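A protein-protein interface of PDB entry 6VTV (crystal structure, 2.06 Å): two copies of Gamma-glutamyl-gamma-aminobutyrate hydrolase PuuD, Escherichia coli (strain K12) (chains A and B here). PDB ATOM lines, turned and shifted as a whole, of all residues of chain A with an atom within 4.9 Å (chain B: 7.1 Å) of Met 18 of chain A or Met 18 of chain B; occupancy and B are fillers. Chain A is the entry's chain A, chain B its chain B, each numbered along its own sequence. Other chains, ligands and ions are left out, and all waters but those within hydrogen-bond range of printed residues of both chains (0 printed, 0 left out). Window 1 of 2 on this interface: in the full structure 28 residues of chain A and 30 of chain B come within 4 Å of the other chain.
The backbone carbonyl oxygen (O) of Gln 29 of chain A sits at hydrogen-bond distance from the backbone NH (N) of Leu 31 of chain B (2.9 Å).
The backbone carbonyl oxygen of Leu 31 of chain A sits at hydrogen-bond distance from the backbone NH of Gln 29 of chain B (2.9 Å).
The backbone NH (N) of Ala 48 of chain A lies within hydrogen-bond range of the backbone carbonyl oxygen (O) of Ala 48 of chain B (2.9 Å).
The backbone NH (N) of Met 18 of chain A sits close to the backbone carbonyl oxygen (O) of Leu 49 of chain A, 3.4 Å away.
O of Met 18 of chain A is in hydrogen-bond range of NE2 of His 51 of chain A (2.8 Å).
The side-chain amide oxygen (OE1) of Gln 29 of chain A lies within hydrogen-bond range of the backbone NH (N) of His 51 of chain A (2.8 Å).
O of Leu 49 of chain B lies close to N of Met 18 of chain B (3.3 Å).
O of Met 18 of chain B lies within hydrogen-bond range of NE2 of His 51 of chain B (2.8 Å).
The backbone NH (N) of His 51 of chain B is in hydrogen-bond range of the side-chain amide oxygen (OE1) of Gln 29 of chain B (2.9 Å).
Met 18 of chain A touches Met 18 of chain B.
Gln 29 of chain A touches Thr 30 of chain B.
Leu 36 of chain B touches Gln 29 of chain A.
Thr 30 of chain A touches Thr 28 of chain B (CB to CG2, 3.6 Å).
Thr 30 of chain A touches Gln 29 of chain B.
Thr 30 of chain A touches Thr 30 of chain B.
Thr 28 of chain B touches Leu 31 of chain A (CG2 to O, 3.4 Å).
Ala 48 of chain A touches Ile 47 of chain B (O to C, 3.8 Å).
CG of Pro 50 of chain A touches CD2 of Leu 36 of chain B (3.5 Å).
Of chain B, only Met 18 (3.5 Å) comes within 4 Å of Met 18 of chain A.
Of the printed residues of chain B, Thr 30 of chain A touches Thr 28 (3.6 Å), Gln 29 (3.4 Å) and Thr 30 (3.96 Å).
Of the printed residues of chain B, Ala 48 of chain A touches Ile 47 (3.8 Å) and Ala 48 (2.9 Å).
Of the printed residues of chain B, Pro 50 of chain A touches Leu 36.
Met 18 of chain B touches just one residue of chain A: Met 18.
Printed residues of chain A within 4 Å of Ile 47 of chain B: Ala 48 (3.8 Å).
Pro 50 of chain B touches none of the printed residues of chain A.
The nearest printed residue of chain A that does not touch Thr 30 of chain B is Leu 31 of chain A (5.1 Å).
Hydrophobic or aromatic side chains of chain B that line the printed part of chain A: Met 18, Leu 36 and Ala 48.
Along chain B the printed residues that touch a printed residue of chain A span positions 18 to 48.
Hydrophobic or aromatic side chains of chain A that line the printed part of chain B: Met 18, Ala 48 and Pro 50.
Among the printed residues, 12 pairs touch across the chains.
Among the printed residues, no Asp or Glu carboxylate lies within 4 Å of a Lys or Arg side-chain nitrogen of the other chain.
Met 18 of chain B touches its own counterpart, Met 18 of chain A.
Gln 29 of chain A touches Thr 30 of chain B, and with the chains exchanged Thr 30 of chain A touches Gln 29 of chain B.
Gln 29 of chain A touches Leu 31 of chain B, and with the chains exchanged Leu 31 of chain A touches Gln 29 of chain B.
Ala 48 of chain A touches its own counterpart, Ala 48 of chain B.
Positions printed for both chains: 16, 17, 18, 19, 20, 29, 30, 31, 48, 49, 50, 51 and 96.
Of the 12 pairs that touch across the chains among the printed residues, 7 have their exchanged pair printed and touching as well.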
ATOM      1  N   VAL A  16     -18.537   9.423   1.755  1.00  0.00           N
ATOM      2  CA  VAL A  16     -19.073   8.119   2.132  1.00  0.00           C
ATOM      3  C   VAL A  16     -19.980   7.628   1.011  1.00  0.00           C
ATOM      4  O   VAL A  16     -20.926   8.321   0.617  1.00  0.00           O
ATOM      5  CB  VAL A  16     -19.831   8.186   3.465  1.00  0.00           C
ATOM      6  CG1 VAL A  16     -20.087   6.790   3.992  1.00  0.00           C
ATOM      7  CG2 VAL A  16     -19.051   9.010   4.479  1.00  0.00           C
ATOM      8  N   VAL A  17     -19.699   6.430   0.509  1.00  0.00           N
ATOM      9  CA  VAL A  17     -20.477   5.849  -0.579  1.00  0.00           C
ATOM     10  C   VAL A  17     -21.793   5.316  -0.026  1.00  0.00           C
ATOM     11  O   VAL A  17     -21.814   4.593   0.978  1.00  0.00           O
ATOM     12  CB  VAL A  17     -19.678   4.741  -1.286  1.00  0.00           C
ATOM     13  CG1 VAL A  17     -20.610   3.788  -2.022  1.00  0.00           C
ATOM     14  CG2 VAL A  17     -18.669   5.353  -2.249  1.00  0.00           C
ATOM     15  N   MET A  18     -22.894   5.673  -0.679  1.00  0.00           N
ATOM     16  CA  MET A  18     -24.211   5.243  -0.242  1.00  0.00           C
ATOM     17  C   MET A  18     -24.637   3.968  -0.967  1.00  0.00           C
ATOM     18  O   MET A  18     -24.027   3.539  -1.949  1.00  0.00           O
ATOM     19  CB  MET A  18     -25.242   6.345  -0.479  1.00  0.00           C
ATOM     20  CG  MET A  18     -24.772   7.739  -0.112  1.00  0.00           C
ATOM     21  SD  MET A  18     -26.090   8.947  -0.334  1.00  0.00           S
ATOM     22  CE  MET A  18     -27.267   8.325   0.854  1.00  0.00           C
ATOM     23  N   CYS A  19     -25.709   3.367  -0.464  1.00  0.00           N
ATOM     24  CA  CYS A  19     -26.330   2.190  -1.051  1.00  0.00           C
ATOM     25  C   CYS A  19     -27.728   2.548  -1.536  1.00  0.00           C
ATOM     26  O   CYS A  19     -28.349   3.500  -1.055  1.00  0.00           O
ATOM     27  CB  CYS A  19     -26.409   1.044  -0.037  1.00  0.00           C
ATOM     28  SG  CYS A  19     -24.822   0.473   0.577  1.00  0.00           S
ATOM     29  N   ARG A  20     -28.229   1.769  -2.490  1.00  0.00           N
ATOM     30  CA  ARG A  20     -29.555   1.991  -3.051  1.00  0.00           C
ATOM     31  C   ARG A  20     -30.556   1.038  -2.409  1.00  0.00           C
ATOM     32  O   ARG A  20     -30.298  -0.166  -2.301  1.00  0.00           O
ATOM     33  CB  ARG A  20     -29.552   1.810  -4.569  1.00  0.00           C
ATOM     34  CG  ARG A  20     -30.919   1.987  -5.212  1.00  0.00           C
ATOM     35  CD  ARG A  20     -30.927   1.455  -6.634  1.00  0.00           C
ATOM     36  NE  ARG A  20     -32.260   1.505  -7.227  1.00  0.00           N
ATOM     37  CZ  ARG A  20     -33.202   0.591  -7.021  1.00  0.00           C
ATOM     38  NH1 ARG A  20     -32.960  -0.449  -6.233  1.00  0.00           N
ATOM     39  NH2 ARG A  20     -34.387   0.715  -7.602  1.00  0.00           N
ATOM     40  N   GLN A  29     -31.347   6.472  -1.942  1.00  0.00           N
ATOM     41  CA  GLN A  29     -29.964   6.320  -1.515  1.00  0.00           C
ATOM     42  C   GLN A  29     -29.916   6.380   0.006  1.00  0.00           C
ATOM     43  O   GLN A  29     -30.505   7.279   0.614  1.00  0.00           O
ATOM     44  CB  GLN A  29     -29.084   7.412  -2.122  1.00  0.00           C
ATOM     45  CG  GLN A  29     -29.227   7.555  -3.625  1.00  0.00           C
ATOM     46  CD  GLN A  29     -28.218   6.726  -4.388  1.00  0.00           C
ATOM     47  OE1 GLN A  29     -27.010   6.884  -4.214  1.00  0.00           O
ATOM     48  NE2 GLN A  29     -28.710   5.834  -5.239  1.00  0.00           N
ATOM     49  N   THR A  30     -29.220   5.423   0.615  1.00  0.00           N
ATOM     50  CA  THR A  30     -29.234   5.257   2.061  1.00  0.00           C
ATOM     51  C   THR A  30     -27.815   5.139   2.601  1.00  0.00           C
ATOM     52  O   THR A  30     -26.880   4.765   1.889  1.00  0.00           O
ATOM     53  CB  THR A  30     -30.039   4.015   2.477  1.00  0.00           C
ATOM     54  OG1 THR A  30     -29.421   2.841   1.936  1.00  0.00           O
ATOM     55  CG2 THR A  30     -31.474   4.109   1.978  1.00  0.00           C
ATOM     56  N   LEU A  31     -27.674   5.456   3.887  1.00  0.00           N
ATOM     57  CA  LEU A  31     -26.392   5.354   4.580  1.00  0.00           C
ATOM     58  C   LEU A  31     -26.679   5.161   6.062  1.00  0.00           C
ATOM     59  O   LEU A  31     -27.223   6.060   6.709  1.00  0.00           O
ATOM     60  CB  LEU A  31     -25.539   6.596   4.341  1.00  0.00           C
ATOM     61  CG  LEU A  31     -24.228   6.699   5.116  1.00  0.00           C
ATOM     62  CD1 LEU A  31     -23.366   5.471   4.869  1.00  0.00           C
ATOM     63  CD2 LEU A  31     -23.492   7.963   4.709  1.00  0.00           C
ATOM     64  N   ALA A  48     -22.360  12.270   2.308  1.00  0.00           N
ATOM     65  CA  ALA A  48     -22.814  11.068   1.622  1.00  0.00           C
ATOM     66  C   ALA A  48     -22.781  11.287   0.114  1.00  0.00           C
ATOM     67  O   ALA A  48     -23.235  12.325  -0.380  1.00  0.00           O
ATOM     68  CB  ALA A  48     -24.220  10.687   2.081  1.00  0.00           C
ATOM     69  N   LEU A  49     -22.245  10.302  -0.615  1.00  0.00           N
ATOM     70  CA  LEU A  49     -22.022  10.441  -2.046  1.00  0.00           C
ATOM     71  C   LEU A  49     -23.063   9.647  -2.818  1.00  0.00           C
ATOM     72  O   LEU A  49     -23.038   8.408  -2.775  1.00  0.00           O
ATOM     73  CB  LEU A  49     -20.618   9.971  -2.412  1.00  0.00           C
ATOM     74  CG  LEU A  49     -19.471  10.589  -1.612  1.00  0.00           C
ATOM     75  CD1 LEU A  49     -18.159   9.918  -1.975  1.00  0.00           C
ATOM     76  CD2 LEU A  49     -19.397  12.089  -1.853  1.00  0.00           C
ATOM     77  N   PRO A  50     -23.979  10.296  -3.532  1.00  0.00           N
ATOM     78  CA  PRO A  50     -24.969   9.554  -4.319  1.00  0.00           C
ATOM     79  C   PRO A  50     -24.336   8.859  -5.514  1.00  0.00           C
ATOM     80  O   PRO A  50     -23.275   9.246  -6.011  1.00  0.00           O
ATOM     81  CB  PRO A  50     -25.956  10.637  -4.771  1.00  0.00           C
ATOM     82  CG  PRO A  50     -25.682  11.816  -3.883  1.00  0.00           C
ATOM     83  CD  PRO A  50     -24.236  11.743  -3.540  1.00  0.00           C
ATOM     84  N   HIS A  51     -25.028   7.815  -5.983  1.00  0.00           N
ATOM     85  CA  HIS A  51     -24.515   7.000  -7.082  1.00  0.00           C
ATOM     86  C   HIS A  51     -24.301   7.816  -8.350  1.00  0.00           C
ATOM     87  O   HIS A  51     -23.409   7.499  -9.146  1.00  0.00           O
ATOM     88  CB  HIS A  51     -25.473   5.843  -7.366  1.00  0.00           C
ATOM     89  CG  HIS A  51     -25.537   4.829  -6.267  1.00  0.00           C
ATOM     90  ND1 HIS A  51     -26.452   3.799  -6.259  1.00  0.00           N
ATOM     91  CD2 HIS A  51     -24.799   4.686  -5.142  1.00  0.00           C
ATOM     92  CE1 HIS A  51     -26.277   3.065  -5.175  1.00  0.00           C
ATOM     93  NE2 HIS A  51     -25.279   3.582  -4.480  1.00  0.00           N
ATOM     94  N   ARG A  96     -24.154   1.391  -6.776  1.00  0.00           N
ATOM     95  CA  ARG A  96     -23.040   1.399  -5.834  1.00  0.00           C
ATOM     96  C   ARG A  96     -21.801   0.759  -6.446  1.00  0.00           C
ATOM     97  O   ARG A  96     -20.680   1.240  -6.245  1.00  0.00           O
ATOM     98  CB  ARG A  96     -23.436   0.680  -4.545  1.00  0.00           C
ATOM     99  CG  ARG A  96     -22.262   0.101  -3.780  1.00  0.00           C
ATOM    100  CD  ARG A  96     -22.308   0.474  -2.313  1.00  0.00           C
ATOM    101  NE  ARG A  96     -21.008   0.299  -1.673  1.00  0.00           N
ATOM    102  CZ  ARG A  96     -20.819   0.303  -0.359  1.00  0.00           C
ATOM    103  NH1 ARG A  96     -21.852   0.467   0.456  1.00  0.00           N
ATOM    104  NH2 ARG A  96     -19.603   0.139   0.143  1.00  0.00           N
ATOM    105  N   VAL B  16     -27.583  18.614   0.001  1.00  0.00           N
ATOM    106  CA  VAL B  16     -28.943  18.092   0.058  1.00  0.00           C
ATOM    107  C   VAL B  16     -29.189  17.534   1.453  1.00  0.00           C
ATOM    108  O   VAL B  16     -28.518  16.586   1.879  1.00  0.00           O
ATOM    109  CB  VAL B  16     -29.183  17.020  -1.015  1.00  0.00           C
ATOM    110  CG1 VAL B  16     -30.665  16.743  -1.149  1.00  0.00           C
ATOM    111  CG2 VAL B  16     -28.601  17.464  -2.347  1.00  0.00           C
ATOM    112  N   VAL B  17     -30.159  18.119   2.157  1.00  0.00           N
ATOM    113  CA  VAL B  17     -30.496  17.668   3.501  1.00  0.00           C
ATOM    114  C   VAL B  17     -31.192  16.317   3.424  1.00  0.00           C
ATOM    115  O   VAL B  17     -32.139  16.128   2.651  1.00  0.00           O
ATOM    116  CB  VAL B  17     -31.370  18.712   4.212  1.00  0.00           C
ATOM    117  CG1 VAL B  17     -31.977  18.129   5.482  1.00  0.00           C
ATOM    118  CG2 VAL B  17     -30.549  19.952   4.536  1.00  0.00           C
ATOM    119  N   MET B  18     -30.725  15.371   4.230  1.00  0.00           N
ATOM    120  CA  MET B  18     -31.257  14.019   4.219  1.00  0.00           C
ATOM    121  C   MET B  18     -32.377  13.863   5.246  1.00  0.00           C
ATOM    122  O   MET B  18     -32.634  14.744   6.069  1.00  0.00           O
ATOM    123  CB  MET B  18     -30.140  13.012   4.493  1.00  0.00           C
ATOM    124  CG  MET B  18     -28.919  13.196   3.614  1.00  0.00           C
ATOM    125  SD  MET B  18     -27.597  12.050   4.043  1.00  0.00           S
ATOM    126  CE  MET B  18     -28.265  10.543   3.361  1.00  0.00           C
ATOM    127  N   CYS B  19     -33.051  12.717   5.182  1.00  0.00           N
ATOM    128  CA  CYS B  19     -34.094  12.345   6.126  1.00  0.00           C
ATOM    129  C   CYS B  19     -33.688  11.080   6.872  1.00  0.00           C
ATOM    130  O   CYS B  19     -32.833  10.314   6.421  1.00  0.00           O
ATOM    131  CB  CYS B  19     -35.441  12.117   5.423  1.00  0.00           C
ATOM    132  SG  CYS B  19     -36.050  13.509   4.460  1.00  0.00           S
ATOM    133  N   ARG B  20     -34.319  10.864   8.020  1.00  0.00           N
ATOM    134  CA  ARG B  20     -34.025   9.714   8.864  1.00  0.00           C
ATOM    135  C   ARG B  20     -35.068   8.625   8.662  1.00  0.00           C
ATOM    136  O   ARG B  20     -36.271   8.900   8.596  1.00  0.00           O
ATOM    137  CB  ARG B  20     -33.977  10.112  10.340  1.00  0.00           C
ATOM    138  CG  ARG B  20     -33.464   9.023  11.279  1.00  0.00           C
ATOM    139  CD  ARG B  20     -33.003   9.646  12.584  1.00  0.00           C
ATOM    140  NE  ARG B  20     -32.085   8.806  13.343  1.00  0.00           N
ATOM    141  CZ  ARG B  20     -32.400   8.208  14.486  1.00  0.00           C
ATOM    142  NH1 ARG B  20     -33.616   8.353  14.996  1.00  0.00           N
ATOM    143  NH2 ARG B  20     -31.504   7.468  15.122  1.00  0.00           N
ATOM    144  N   THR B  28     -30.979   5.099   9.735  1.00  0.00           N
ATOM    145  CA  THR B  28     -30.385   5.329   8.427  1.00  0.00           C
ATOM    146  C   THR B  28     -30.729   6.728   7.942  1.00  0.00           C
ATOM    147  O   THR B  28     -31.849   7.207   8.142  1.00  0.00           O
ATOM    148  CB  THR B  28     -30.876   4.288   7.409  1.00  0.00           C
ATOM    149  OG1 THR B  28     -30.663   2.971   7.931  1.00  0.00           O
ATOM    150  CG2 THR B  28     -30.126   4.426   6.096  1.00  0.00           C
ATOM    151  N   GLN B  29     -29.754   7.380   7.316  1.00  0.00           N
ATOM    152  CA  GLN B  29     -29.976   8.644   6.628  1.00  0.00           C
ATOM    153  C   GLN B  29     -30.288   8.356   5.166  1.00  0.00           C
ATOM    154  O   GLN B  29     -29.563   7.604   4.506  1.00  0.00           O
ATOM    155  CB  GLN B  29     -28.750   9.547   6.752  1.00  0.00           C
ATOM    156  CG  GLN B  29     -28.403   9.917   8.185  1.00  0.00           C
ATOM    157  CD  GLN B  29     -29.234  11.076   8.698  1.00  0.00           C
ATOM    158  OE1 GLN B  29     -29.150  12.190   8.180  1.00  0.00           O
ATOM    159  NE2 GLN B  29     -30.041  10.821   9.722  1.00  0.00           N
ATOM    160  N   THR B  30     -31.371   8.946   4.663  1.00  0.00           N
ATOM    161  CA  THR B  30     -31.895   8.600   3.349  1.00  0.00           C
ATOM    162  C   THR B  30     -32.070   9.844   2.489  1.00  0.00           C
ATOM    163  O   THR B  30     -32.205  10.965   2.988  1.00  0.00           O
ATOM    164  CB  THR B  30     -33.242   7.868   3.456  1.00  0.00           C
ATOM    165  OG1 THR B  30     -34.254   8.787   3.882  1.00  0.00           O
ATOM    166  CG2 THR B  30     -33.153   6.715   4.449  1.00  0.00           C
ATOM    167  N   LEU B  31     -32.075   9.620   1.177  1.00  0.00           N
ATOM    168  CA  LEU B  31     -32.340  10.669   0.200  1.00  0.00           C
ATOM    169  C   LEU B  31     -32.926  10.017  -1.041  1.00  0.00           C
ATOM    170  O   LEU B  31     -32.248   9.223  -1.700  1.00  0.00           O
ATOM    171  CB  LEU B  31     -31.066  11.441  -0.146  1.00  0.00           C
ATOM    172  CG  LEU B  31     -31.205  12.517  -1.224  1.00  0.00           C
ATOM    173  CD1 LEU B  31     -32.316  13.493  -0.870  1.00  0.00           C
ATOM    174  CD2 LEU B  31     -29.886  13.242  -1.410  1.00  0.00           C
ATOM    175  N   LEU B  36     -32.448  13.654  -6.369  1.00  0.00           N
ATOM    176  CA  LEU B  36     -31.097  13.700  -6.915  1.00  0.00           C
ATOM    177  C   LEU B  36     -31.114  13.834  -8.430  1.00  0.00           C
ATOM    178  O   LEU B  36     -30.333  14.606  -8.998  1.00  0.00           O
ATOM    179  CB  LEU B  36     -30.329  12.445  -6.504  1.00  0.00           C
ATOM    180  CG  LEU B  36     -29.882  12.417  -5.047  1.00  0.00           C
ATOM    181  CD1 LEU B  36     -29.522  11.005  -4.625  1.00  0.00           C
ATOM    182  CD2 LEU B  36     -28.711  13.359  -4.858  1.00  0.00           C
ATOM    183  N   ILE B  47     -24.381  16.589  -3.022  1.00  0.00           N
ATOM    184  CA  ILE B  47     -23.807  15.813  -1.932  1.00  0.00           C
ATOM    185  C   ILE B  47     -24.822  15.795  -0.797  1.00  0.00           C
ATOM    186  O   ILE B  47     -25.391  16.835  -0.450  1.00  0.00           O
ATOM    187  CB  ILE B  47     -22.451  16.375  -1.460  1.00  0.00           C
ATOM    188  CG1 ILE B  47     -22.564  17.855  -1.089  1.00  0.00           C
ATOM    189  CG2 ILE B  47     -21.388  16.176  -2.533  1.00  0.00           C
ATOM    190  CD1 ILE B  47     -21.367  18.378  -0.324  1.00  0.00           C
ATOM    191  N   ALA B  48     -25.069  14.613  -0.242  1.00  0.00           N
ATOM    192  CA  ALA B  48     -26.089  14.448   0.783  1.00  0.00           C
ATOM    193  C   ALA B  48     -25.512  14.760   2.157  1.00  0.00           C
ATOM    194  O   ALA B  48     -24.394  14.350   2.485  1.00  0.00           O
ATOM    195  CB  ALA B  48     -26.660  13.030   0.752  1.00  0.00           C
ATOM    196  N   LEU B  49     -26.287  15.486   2.960  1.00  0.00           N
ATOM    197  CA  LEU B  49     -25.820  15.983   4.249  1.00  0.00           C
ATOM    198  C   LEU B  49     -26.496  15.235   5.388  1.00  0.00           C
ATOM    199  O   LEU B  49     -27.711  15.387   5.588  1.00  0.00           O
ATOM    200  CB  LEU B  49     -26.091  17.484   4.366  1.00  0.00           C
ATOM    201  CG  LEU B  49     -25.643  18.339   3.179  1.00  0.00           C
ATOM    202  CD1 LEU B  49     -26.095  19.782   3.354  1.00  0.00           C
ATOM    203  CD2 LEU B  49     -24.135  18.260   2.995  1.00  0.00           C
ATOM    204  N   PRO B  50     -25.766  14.430   6.158  1.00  0.00           N
ATOM    205  CA  PRO B  50     -26.371  13.760   7.314  1.00  0.00           C
ATOM    206  C   PRO B  50     -26.699  14.742   8.428  1.00  0.00           C
ATOM    207  O   PRO B  50     -26.154  15.844   8.513  1.00  0.00           O
ATOM    208  CB  PRO B  50     -25.295  12.762   7.762  1.00  0.00           C
ATOM    209  CG  PRO B  50     -24.277  12.732   6.662  1.00  0.00           C
ATOM    210  CD  PRO B  50     -24.362  14.042   5.958  1.00  0.00           C
ATOM    211  N   HIS B  51     -27.605  14.304   9.309  1.00  0.00           N
ATOM    212  CA  HIS B  51     -28.084  15.152  10.395  1.00  0.00           C
ATOM    213  C   HIS B  51     -26.989  15.495  11.395  1.00  0.00           C
ATOM    214  O   HIS B  51     -27.095  16.517  12.082  1.00  0.00           O
ATOM    215  CB  HIS B  51     -29.248  14.470  11.117  1.00  0.00           C
ATOM    216  CG  HIS B  51     -30.458  14.273  10.258  1.00  0.00           C
ATOM    217  ND1 HIS B  51     -31.524  13.488  10.642  1.00  0.00           N
ATOM    218  CD2 HIS B  51     -30.770  14.756   9.032  1.00  0.00           C
ATOM    219  CE1 HIS B  51     -32.441  13.496   9.692  1.00  0.00           C
ATOM    220  NE2 HIS B  51     -32.009  14.257   8.703  1.00  0.00           N
ATOM    221  N   TYR B  70     -30.319  22.460  -0.803  1.00  0.00           N
ATOM    222  CA  TYR B  70     -31.433  21.750  -1.424  1.00  0.00           C
ATOM    223  C   TYR B  70     -32.221  21.053  -0.324  1.00  0.00           C
ATOM    224  O   TYR B  70     -31.700  20.152   0.342  1.00  0.00           O
ATOM    225  CB  TYR B  70     -30.912  20.749  -2.457  1.00  0.00           C
ATOM    226  CG  TYR B  70     -31.956  20.045  -3.294  1.00  0.00           C
ATOM    227  CD1 TYR B  70     -33.134  20.679  -3.669  1.00  0.00           C
ATOM    228  CD2 TYR B  70     -31.746  18.744  -3.732  1.00  0.00           C
ATOM    229  CE1 TYR B  70     -34.079  20.025  -4.446  1.00  0.00           C
ATOM    230  CE2 TYR B  70     -32.680  18.084  -4.500  1.00  0.00           C
ATOM    231  CZ  TYR B  70     -33.842  18.727  -4.859  1.00  0.00           C
ATOM    232  OH  TYR B  70     -34.768  18.061  -5.632  1.00  0.00           O
ATOM    233  N   PRO B  72     -35.229  18.730   0.242  1.00  0.00           N
ATOM    234  CA  PRO B  72     -36.252  17.870  -0.357  1.00  0.00           C
ATOM    235  C   PRO B  72     -37.485  17.764   0.527  1.00  0.00           C
ATOM    236  O   PRO B  72     -37.469  18.088   1.716  1.00  0.00           O
ATOM    237  CB  PRO B  72     -35.554  16.509  -0.486  1.00  0.00           C
ATOM    238  CG  PRO B  72     -34.097  16.772  -0.226  1.00  0.00           C
ATOM    239  CD  PRO B  72     -34.049  17.964   0.671  1.00  0.00           C
ATOM    240  N   SER B  74     -40.557  15.306   2.235  1.00  0.00           N
ATOM    241  CA  SER B  74     -40.505  14.105   3.059  1.00  0.00           C
ATOM    242  C   SER B  74     -41.869  13.864   3.694  1.00  0.00           C
ATOM    243  O   SER B  74     -42.623  14.820   3.916  1.00  0.00           O
ATOM    244  CB  SER B  74     -39.428  14.242   4.138  1.00  0.00           C
ATOM    245  OG  SER B  74     -39.378  13.102   4.980  1.00  0.00           O
ATOM    246  N   ASP B  93     -39.299  14.087  12.472  1.00  0.00           N
ATOM    247  CA  ASP B  93     -37.881  13.867  12.182  1.00  0.00           C
ATOM    248  C   ASP B  93     -37.101  14.975  12.870  1.00  0.00           C
ATOM    249  O   ASP B  93     -36.666  15.942  12.232  1.00  0.00           O
ATOM    250  CB  ASP B  93     -37.621  13.844  10.673  1.00  0.00           C
ATOM    251  CG  ASP B  93     -36.214  13.378  10.322  1.00  0.00           C
ATOM    252  OD1 ASP B  93     -35.987  13.024   9.144  1.00  0.00           O
ATOM    253  OD2 ASP B  93     -35.340  13.354  11.212  1.00  0.00           O
ATOM    254  N   GLY B  95     -34.109  15.182  13.950  1.00  0.00           N
ATOM    255  CA  GLY B  95     -32.770  15.393  13.425  1.00  0.00           C
ATOM    256  C   GLY B  95     -32.759  16.262  12.183  1.00  0.00           C
ATOM    257  O   GLY B  95     -31.933  17.169  12.057  1.00  0.00           O
ATOM    258  N   ARG B  96     -33.679  16.001  11.249  1.00  0.00           N
ATOM    259  CA  ARG B  96     -33.775  16.848  10.065  1.00  0.00           C
ATOM    260  C   ARG B  96     -34.192  18.265  10.435  1.00  0.00           C
ATOM    261  O   ARG B  96     -33.670  19.235   9.874  1.00  0.00           O
ATOM    262  CB  ARG B  96     -34.753  16.247   9.055  1.00  0.00           C
ATOM    263  CG  ARG B  96     -35.306  17.279   8.084  1.00  0.00           C
ATOM    264  CD  ARG B  96     -35.440  16.751   6.671  1.00  0.00           C
ATOM    265  NE  ARG B  96     -35.794  17.828   5.751  1.00  0.00           N
ATOM    266  CZ  ARG B  96     -36.082  17.657   4.465  1.00  0.00           C
ATOM    267  NH1 ARG B  96     -36.062  16.444   3.934  1.00  0.00           N
ATOM    268  NH2 ARG B  96     -36.391  18.704   3.711  1.00  0.00           N
ATOM    269  N   ASP B  97     -35.136  18.401  11.372  1.00  0.00           N
ATOM    270  CA  ASP B  97     -35.508  19.718  11.879  1.00  0.00           C
ATOM    271  C   ASP B  97     -34.281  20.489  12.345  1.00  0.00           C
ATOM    272  O   ASP B  97     -34.097  21.662  12.000  1.00  0.00           O
ATOM    273  CB  ASP B  97     -36.505  19.574  13.030  1.00  0.00           C
ATOM    274  CG  ASP B  97     -37.911  19.274  12.557  1.00  0.00           C
ATOM    275  OD1 ASP B  97     -38.137  19.215  11.329  1.00  0.00           O
ATOM    276  OD2 ASP B  97     -38.795  19.094  13.423  1.00  0.00           O
ATOM    277  N   LEU B  99     -31.045  20.063  11.552  1.00  0.00           N
ATOM    278  CA  LEU B  99     -30.163  20.417  10.445  1.00  0.00           C
ATOM    279  C   LEU B  99     -30.801  21.459   9.534  1.00  0.00           C
ATOM    280  O   LEU B  99     -30.130  22.399   9.092  1.00  0.00           O
ATOM    281  CB  LEU B  99     -29.789  19.166   9.649  1.00  0.00           C
ATOM    282  CG  LEU B  99     -28.914  19.396   8.414  1.00  0.00           C
ATOM    283  CD1 LEU B  99     -27.579  20.011   8.806  1.00  0.00           C
ATOM    284  CD2 LEU B  99     -28.706  18.101   7.633  1.00  0.00           C
ATOM    285  N   SER B 100     -32.097  21.311   9.244  1.00  0.00           N
ATOM    286  CA  SER B 100     -32.769  22.237   8.337  1.00  0.00           C
ATOM    287  C   SER B 100     -32.779  23.652   8.897  1.00  0.00           C
ATOM    288  O   SER B 100     -32.449  24.612   8.192  1.00  0.00           O
ATOM    289  CB  SER B 100     -34.196  21.762   8.065  1.00  0.00           C
ATOM    290  OG  SER B 100     -34.198  20.550   7.330  1.00  0.00           O
ATOM    291  N   GLU B 123     -40.226  24.117   6.128  1.00  0.00           N
ATOM    292  CA  GLU B 123     -39.035  24.445   6.902  1.00  0.00           C
ATOM    293  C   GLU B 123     -38.647  25.908   6.719  1.00  0.00           C
ATOM    294  O   GLU B 123     -38.252  26.576   7.681  1.00  0.00           O
ATOM    295  CB  GLU B 123     -37.880  23.525   6.504  1.00  0.00           C
ATOM    296  CG  GLU B 123     -38.015  22.108   7.034  1.00  0.00           C
ATOM    297  CD  GLU B 123     -37.047  21.142   6.379  1.00  0.00           C
ATOM    298  OE1 GLU B 123     -36.500  21.476   5.307  1.00  0.00           O
ATOM    299  OE2 GLU B 123     -36.830  20.047   6.937  1.00  0.00           O
